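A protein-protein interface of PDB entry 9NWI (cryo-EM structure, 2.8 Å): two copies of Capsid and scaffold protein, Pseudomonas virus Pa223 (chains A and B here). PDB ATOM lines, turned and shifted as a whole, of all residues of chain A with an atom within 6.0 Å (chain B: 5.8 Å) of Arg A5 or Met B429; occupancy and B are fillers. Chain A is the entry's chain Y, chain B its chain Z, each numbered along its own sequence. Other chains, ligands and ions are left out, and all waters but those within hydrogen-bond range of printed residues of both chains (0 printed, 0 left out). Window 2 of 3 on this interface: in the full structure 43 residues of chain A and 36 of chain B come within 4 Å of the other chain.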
ATOM      1  N   LEU A   3     -25.097 -24.613  22.347  1.00  0.00           N
ATOM      2  CA  LEU A   3     -26.331 -25.386  22.455  1.00  0.00           C
ATOM      3  C   LEU A   3     -26.022 -26.808  22.013  1.00  0.00           C
ATOM      4  O   LEU A   3     -25.678 -27.032  20.850  1.00  0.00           O
ATOM      5  CB  LEU A   3     -27.438 -24.774  21.605  1.00  0.00           C
ATOM      6  CG  LEU A   3     -28.361 -23.767  22.291  1.00  0.00           C
ATOM      7  CD1 LEU A   3     -29.642 -23.591  21.498  1.00  0.00           C
ATOM      8  CD2 LEU A   3     -28.670 -24.201  23.709  1.00  0.00           C
ATOM      9  N   GLU A   4     -26.138 -27.760  22.931  1.00  0.00           N
ATOM     10  CA  GLU A   4     -25.850 -29.150  22.613  1.00  0.00           C
ATOM     11  C   GLU A   4     -27.101 -29.839  22.088  1.00  0.00           C
ATOM     12  O   GLU A   4     -28.226 -29.455  22.412  1.00  0.00           O
ATOM     13  CB  GLU A   4     -25.321 -29.890  23.840  1.00  0.00           C
ATOM     14  CG  GLU A   4     -24.023 -29.325  24.391  1.00  0.00           C
ATOM     15  CD  GLU A   4     -22.796 -29.866  23.680  1.00  0.00           C
ATOM     16  OE1 GLU A   4     -22.945 -30.455  22.588  1.00  0.00           O
ATOM     17  OE2 GLU A   4     -21.678 -29.702  24.213  1.00  0.00           O
ATOM     18  N   ARG A   5     -26.895 -30.862  21.264  1.00  0.00           N
ATOM     19  CA  ARG A   5     -27.994 -31.597  20.659  1.00  0.00           C
ATOM     20  C   ARG A   5     -27.738 -33.091  20.760  1.00  0.00           C
ATOM     21  O   ARG A   5     -26.629 -33.560  20.494  1.00  0.00           O
ATOM     22  CB  ARG A   5     -28.188 -31.196  19.197  1.00  0.00           C
ATOM     23  CG  ARG A   5     -29.282 -30.168  18.987  1.00  0.00           C
ATOM     24  CD  ARG A   5     -29.284 -29.643  17.565  1.00  0.00           C
ATOM     25  NE  ARG A   5     -27.961 -29.200  17.147  1.00  0.00           N
ATOM     26  CZ  ARG A   5     -27.495 -27.971  17.320  1.00  0.00           C
ATOM     27  NH1 ARG A   5     -28.222 -27.033  17.904  1.00  0.00           N
ATOM     28  NH2 ARG A   5     -26.270 -27.677  16.899  1.00  0.00           N
ATOM     29  N   GLN A   6     -28.772 -33.833  21.146  1.00  0.00           N
ATOM     30  CA  GLN A   6     -28.713 -35.287  21.209  1.00  0.00           C
ATOM     31  C   GLN A   6     -29.871 -35.857  20.407  1.00  0.00           C
ATOM     32  O   GLN A   6     -31.026 -35.502  20.648  1.00  0.00           O
ATOM     33  CB  GLN A   6     -28.771 -35.785  22.653  1.00  0.00           C
ATOM     34  CG  GLN A   6     -28.930 -37.284  22.776  1.00  0.00           C
ATOM     35  CD  GLN A   6     -27.702 -38.036  22.318  1.00  0.00           C
ATOM     36  OE1 GLN A   6     -26.698 -38.096  23.025  1.00  0.00           O
ATOM     37  NE2 GLN A   6     -27.774 -38.613  21.126  1.00  0.00           N
ATOM     38  N   GLU A   7     -29.567 -36.746  19.468  1.00  0.00           N
ATOM     39  CA  GLU A   7     -30.558 -37.270  18.539  1.00  0.00           C
ATOM     40  C   GLU A   7     -30.869 -38.722  18.869  1.00  0.00           C
ATOM     41  O   GLU A   7     -29.955 -39.539  19.010  1.00  0.00           O
ATOM     42  CB  GLU A   7     -30.063 -37.153  17.099  1.00  0.00           C
ATOM     43  CG  GLU A   7     -30.748 -38.097  16.134  1.00  0.00           C
ATOM     44  CD  GLU A   7     -30.754 -37.572  14.714  1.00  0.00           C
ATOM     45  OE1 GLU A   7     -29.664 -37.261  14.191  1.00  0.00           O
ATOM     46  OE2 GLU A   7     -31.847 -37.469  14.121  1.00  0.00           O
ATOM     47  N   ILE A 437     -37.328 -31.441  19.253  1.00  0.00           N
ATOM     48  CA  ILE A 437     -37.610 -31.456  17.824  1.00  0.00           C
ATOM     49  C   ILE A 437     -38.123 -32.849  17.469  1.00  0.00           C
ATOM     50  O   ILE A 437     -37.334 -33.803  17.424  1.00  0.00           O
ATOM     51  CB  ILE A 437     -36.367 -31.097  17.000  1.00  0.00           C
ATOM     52  CG1 ILE A 437     -35.869 -29.703  17.367  1.00  0.00           C
ATOM     53  CG2 ILE A 437     -36.675 -31.175  15.519  1.00  0.00           C
ATOM     54  CD1 ILE A 437     -34.391 -29.644  17.650  1.00  0.00           C
ATOM     55  N   THR A 503     -35.154 -35.229  18.695  1.00  0.00           N
ATOM     56  CA  THR A 503     -33.902 -34.593  19.071  1.00  0.00           C
ATOM     57  C   THR A 503     -34.135 -33.690  20.273  1.00  0.00           C
ATOM     58  O   THR A 503     -35.155 -33.001  20.351  1.00  0.00           O
ATOM     59  CB  THR A 503     -33.323 -33.782  17.903  1.00  0.00           C
ATOM     60  OG1 THR A 503     -32.993 -34.667  16.828  1.00  0.00           O
ATOM     61  CG2 THR A 503     -32.071 -33.040  18.325  1.00  0.00           C
ATOM     62  N   ILE A 504     -33.191 -33.701  21.209  1.00  0.00           N
ATOM     63  CA  ILE A 504     -33.237 -32.869  22.405  1.00  0.00           C
ATOM     64  C   ILE A 504     -32.150 -31.812  22.291  1.00  0.00           C
ATOM     65  O   ILE A 504     -30.980 -32.139  22.056  1.00  0.00           O
ATOM     66  CB  ILE A 504     -33.045 -33.705  23.680  1.00  0.00           C
ATOM     67  CG1 ILE A 504     -33.914 -34.958  23.633  1.00  0.00           C
ATOM     68  CG2 ILE A 504     -33.368 -32.880  24.907  1.00  0.00           C
ATOM     69  CD1 ILE A 504     -33.660 -35.906  24.776  1.00  0.00           C
ATOM     70  N   GLU A 505     -32.534 -30.548  22.458  1.00  0.00           N
ATOM     71  CA  GLU A 505     -31.608 -29.425  22.430  1.00  0.00           C
ATOM     72  C   GLU A 505     -31.483 -28.868  23.840  1.00  0.00           C
ATOM     73  O   GLU A 505     -32.481 -28.440  24.432  1.00  0.00           O
ATOM     74  CB  GLU A 505     -32.090 -28.346  21.463  1.00  0.00           C
ATOM     75  CG  GLU A 505     -31.065 -27.271  21.181  1.00  0.00           C
ATOM     76  CD  GLU A 505     -31.500 -26.335  20.075  1.00  0.00           C
ATOM     77  OE1 GLU A 505     -32.467 -25.576  20.283  1.00  0.00           O
ATOM     78  OE2 GLU A 505     -30.878 -26.362  18.992  1.00  0.00           O
ATOM     79  N   MET A 506     -30.259 -28.858  24.361  1.00  0.00           N
ATOM     80  CA  MET A 506     -29.990 -28.537  25.754  1.00  0.00           C
ATOM     81  C   MET A 506     -29.022 -27.369  25.863  1.00  0.00           C
ATOM     82  O   MET A 506     -28.055 -27.270  25.100  1.00  0.00           O
ATOM     83  CB  MET A 506     -29.411 -29.745  26.491  1.00  0.00           C
ATOM     84  CG  MET A 506     -30.348 -30.930  26.575  1.00  0.00           C
ATOM     85  SD  MET A 506     -29.472 -32.496  26.449  1.00  0.00           S
ATOM     86  CE  MET A 506     -28.001 -32.130  27.396  1.00  0.00           C
ATOM     87  N   ASP B 426     -26.726 -33.514  10.745  1.00  0.00           N
ATOM     88  CA  ASP B 426     -26.944 -32.214  11.378  1.00  0.00           C
ATOM     89  C   ASP B 426     -28.322 -31.716  10.960  1.00  0.00           C
ATOM     90  O   ASP B 426     -28.500 -31.243   9.833  1.00  0.00           O
ATOM     91  CB  ASP B 426     -25.856 -31.224  10.989  1.00  0.00           C
ATOM     92  CG  ASP B 426     -26.155 -29.821  11.465  1.00  0.00           C
ATOM     93  OD1 ASP B 426     -25.794 -29.490  12.614  1.00  0.00           O
ATOM     94  OD2 ASP B 426     -26.760 -29.052  10.693  1.00  0.00           O
ATOM     95  N   ASP B 427     -29.292 -31.810  11.866  1.00  0.00           N
ATOM     96  CA  ASP B 427     -30.676 -31.466  11.565  1.00  0.00           C
ATOM     97  C   ASP B 427     -31.104 -30.158  12.221  1.00  0.00           C
ATOM     98  O   ASP B 427     -32.292 -29.943  12.469  1.00  0.00           O
ATOM     99  CB  ASP B 427     -31.606 -32.602  11.980  1.00  0.00           C
ATOM    100  CG  ASP B 427     -31.714 -32.748  13.478  1.00  0.00           C
ATOM    101  OD1 ASP B 427     -30.679 -32.615  14.162  1.00  0.00           O
ATOM    102  OD2 ASP B 427     -32.832 -32.999  13.973  1.00  0.00           O
ATOM    103  N   ARG B 428     -30.152 -29.274  12.510  1.00  0.00           N
ATOM    104  CA  ARG B 428     -30.474 -27.950  13.027  1.00  0.00           C
ATOM    105  C   ARG B 428     -30.018 -26.839  12.098  1.00  0.00           C
ATOM    106  O   ARG B 428     -30.821 -25.972  11.736  1.00  0.00           O
ATOM    107  CB  ARG B 428     -29.857 -27.756  14.419  1.00  0.00           C
ATOM    108  CG  ARG B 428     -30.391 -26.542  15.154  1.00  0.00           C
ATOM    109  CD  ARG B 428     -31.907 -26.537  15.144  1.00  0.00           C
ATOM    110  NE  ARG B 428     -32.462 -25.190  15.172  1.00  0.00           N
ATOM    111  CZ  ARG B 428     -32.645 -24.478  16.274  1.00  0.00           C
ATOM    112  NH1 ARG B 428     -32.319 -24.952  17.464  1.00  0.00           N
ATOM    113  NH2 ARG B 428     -33.172 -23.261  16.181  1.00  0.00           N
ATOM    114  N   MET B 429     -28.752 -26.841  11.696  1.00  0.00           N
ATOM    115  CA  MET B 429     -28.232 -25.802  10.822  1.00  0.00           C
ATOM    116  C   MET B 429     -28.821 -25.934   9.422  1.00  0.00           C
ATOM    117  O   MET B 429     -29.340 -26.980   9.030  1.00  0.00           O
ATOM    118  CB  MET B 429     -26.708 -25.882  10.743  1.00  0.00           C
ATOM    119  CG  MET B 429     -25.983 -25.699  12.064  1.00  0.00           C
ATOM    120  SD  MET B 429     -26.367 -24.150  12.889  1.00  0.00           S
ATOM    121  CE  MET B 429     -25.916 -24.546  14.573  1.00  0.00           C
ATOM    122  N   MET B 430     -28.735 -24.847   8.663  1.00  0.00           N
ATOM    123  CA  MET B 430     -29.157 -24.830   7.272  1.00  0.00           C
ATOM    124  C   MET B 430     -27.943 -24.962   6.365  1.00  0.00           C
ATOM    125  O   MET B 430     -26.944 -24.261   6.541  1.00  0.00           O
ATOM    126  CB  MET B 430     -29.913 -23.543   6.942  1.00  0.00           C
ATOM    127  CG  MET B 430     -30.895 -23.113   8.010  1.00  0.00           C
ATOM    128  SD  MET B 430     -32.587 -23.592   7.626  1.00  0.00           S
ATOM    129  CE  MET B 430     -32.745 -22.939   5.970  1.00  0.00           C
ATOM    130  N   LYS B 431     -28.033 -25.866   5.397  1.00  0.00           N
ATOM    131  CA  LYS B 431     -26.948 -26.104   4.462  1.00  0.00           C
ATOM    132  C   LYS B 431     -27.062 -25.167   3.265  1.00  0.00           C
ATOM    133  O   LYS B 431     -28.086 -24.516   3.049  1.00  0.00           O
ATOM    134  CB  LYS B 431     -26.949 -27.563   4.016  1.00  0.00           C
ATOM    135  CG  LYS B 431     -26.514 -28.525   5.104  1.00  0.00           C
ATOM    136  CD  LYS B 431     -27.681 -29.351   5.607  1.00  0.00           C
ATOM    137  CE  LYS B 431     -27.423 -29.854   7.013  1.00  0.00           C
ATOM    138  NZ  LYS B 431     -28.621 -29.711   7.879  1.00  0.00           N
ATOM    139  N   GLY B 482     -31.171 -24.595   2.602  1.00  0.00           N
ATOM    140  CA  GLY B 482     -32.256 -25.369   3.176  1.00  0.00           C
ATOM    141  C   GLY B 482     -31.747 -26.249   4.293  1.00  0.00           C
ATOM    142  O   GLY B 482     -30.544 -26.325   4.556  1.00  0.00           O
ATOM    143  N   ARG B 483     -32.689 -26.921   4.952  1.00  0.00           N
ATOM    144  CA  ARG B 483     -32.353 -27.788   6.072  1.00  0.00           C
ATOM    145  C   ARG B 483     -32.180 -29.241   5.641  1.00  0.00           C
ATOM    146  O   ARG B 483     -31.189 -29.882   6.000  1.00  0.00           O
ATOM    147  CB  ARG B 483     -33.423 -27.683   7.159  1.00  0.00           C
ATOM    148  CG  ARG B 483     -32.963 -28.169   8.519  1.00  0.00           C
ATOM    149  CD  ARG B 483     -34.012 -27.913   9.580  1.00  0.00           C
ATOM    150  NE  ARG B 483     -33.743 -26.695  10.334  1.00  0.00           N
ATOM    151  CZ  ARG B 483     -34.644 -25.756  10.584  1.00  0.00           C
ATOM    152  NH1 ARG B 483     -35.889 -25.863  10.154  1.00  0.00           N
ATOM    153  NH2 ARG B 483     -34.287 -24.685  11.284  1.00  0.00           N
ATOM    154  N   LYS B 509     -22.233 -23.167   6.546  1.00  0.00           N
ATOM    155  CA  LYS B 509     -23.634 -23.126   6.940  1.00  0.00           C
ATOM    156  C   LYS B 509     -24.129 -21.688   7.069  1.00  0.00           C
ATOM    157  O   LYS B 509     -23.352 -20.738   7.186  1.00  0.00           O
ATOM    158  CB  LYS B 509     -23.830 -23.875   8.256  1.00  0.00           C
ATOM    159  CG  LYS B 509     -23.938 -25.378   8.089  1.00  0.00           C
ATOM    160  CD  LYS B 509     -23.430 -26.109   9.316  1.00  0.00           C
ATOM    161  CE  LYS B 509     -23.243 -27.586   9.033  1.00  0.00           C
ATOM    162  NZ  LYS B 509     -22.701 -27.817   7.670  1.00  0.00           N
ATOM    163  N   GLY B 511     -26.708 -20.348   9.309  1.00  0.00           N
ATOM    164  CA  GLY B 511     -27.566 -20.175  10.465  1.00  0.00           C
ATOM    165  C   GLY B 511     -28.456 -21.378  10.693  1.00  0.00           C
ATOM    166  O   GLY B 511     -28.451 -22.356   9.940  1.00  0.00           O
ATOM    167  N   MET B 512     -29.240 -21.301  11.767  1.00  0.00           N
ATOM    168  CA  MET B 512     -30.106 -22.405  12.150  1.00  0.00           C
ATOM    169  C   MET B 512     -31.574 -22.035  12.307  1.00  0.00           C
ATOM    170  O   MET B 512     -32.321 -22.779  12.953  1.00  0.00           O
ATOM    171  CB  MET B 512     -29.560 -23.085  13.418  1.00  0.00           C
ATOM    172  CG  MET B 512     -29.991 -22.571  14.782  1.00  0.00           C
ATOM    173  SD  MET B 512     -29.064 -21.121  15.298  1.00  0.00           S
ATOM    174  CE  MET B 512     -29.402 -21.142  17.054  1.00  0.00           C
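No position is printed for both chains.
The side-chain carboxylate of Glu A505 is in salt-bridge range of the guanidinium group of Arg B428 (2.5 Å). The side-chain hydroxyl (OG1) of Thr A503 is in hydrogen-bond range of the side-chain carboxylate (OD2) of Asp B427.
NE of Arg B428 is in hydrogen-bond range of O of Met B512, at 3.3 Å. The backbone carbonyl oxygen of Arg B428 lies within hydrogen-bond range of the guanidinium group of Arg B483 (3.3 Å). The side-chain carboxylate (OD2) of Asp B426 sits at hydrogen-bond distance from the backbone NH (N) of Met B429 (3.1 Å). The side-chain carboxylate of Glu A505 is in salt-bridge range of the guanidinium group of Arg A5, 2.9 Å away. The backbone carbonyl oxygen of Thr A503 sits at hydrogen-bond distance from the backbone NH of Ile A437 (2.9 Å). The backbone carbonyl oxygen (O) of Met B429 lies within hydrogen-bond range of the side-chain amino group (NZ) of Lys B431, 3.0 Å away.
Arg A5 touches two residues of chain B. Printed residues of chain B within 4 Å of Thr A503: Asp B427 (3.3 Å). Of the printed residues of chain B, Glu A505 touches Arg B428 (2.5 Å). Of the printed residues of chain A, Asp B427 touches Thr A503. Printed residues of chain A within 4 Å of Met B429: Arg A5. The nearest residue of chain B that does not touch Arg A5 is Asp B426 (4.7 Å). The nearest printed residue of chain A that does not touch Met B429 is Leu A3 (6.8 Å).
Among the printed residues, merely in contact across the chains: Arg A5 with Arg B428 (3.5 Å) and Arg A5 with Met B429 (3.9 Å).
Of the 11 printed residues of chain B, 3 touch a printed residue of chain A. Among the printed residues, 4 pairs touch across the chains.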
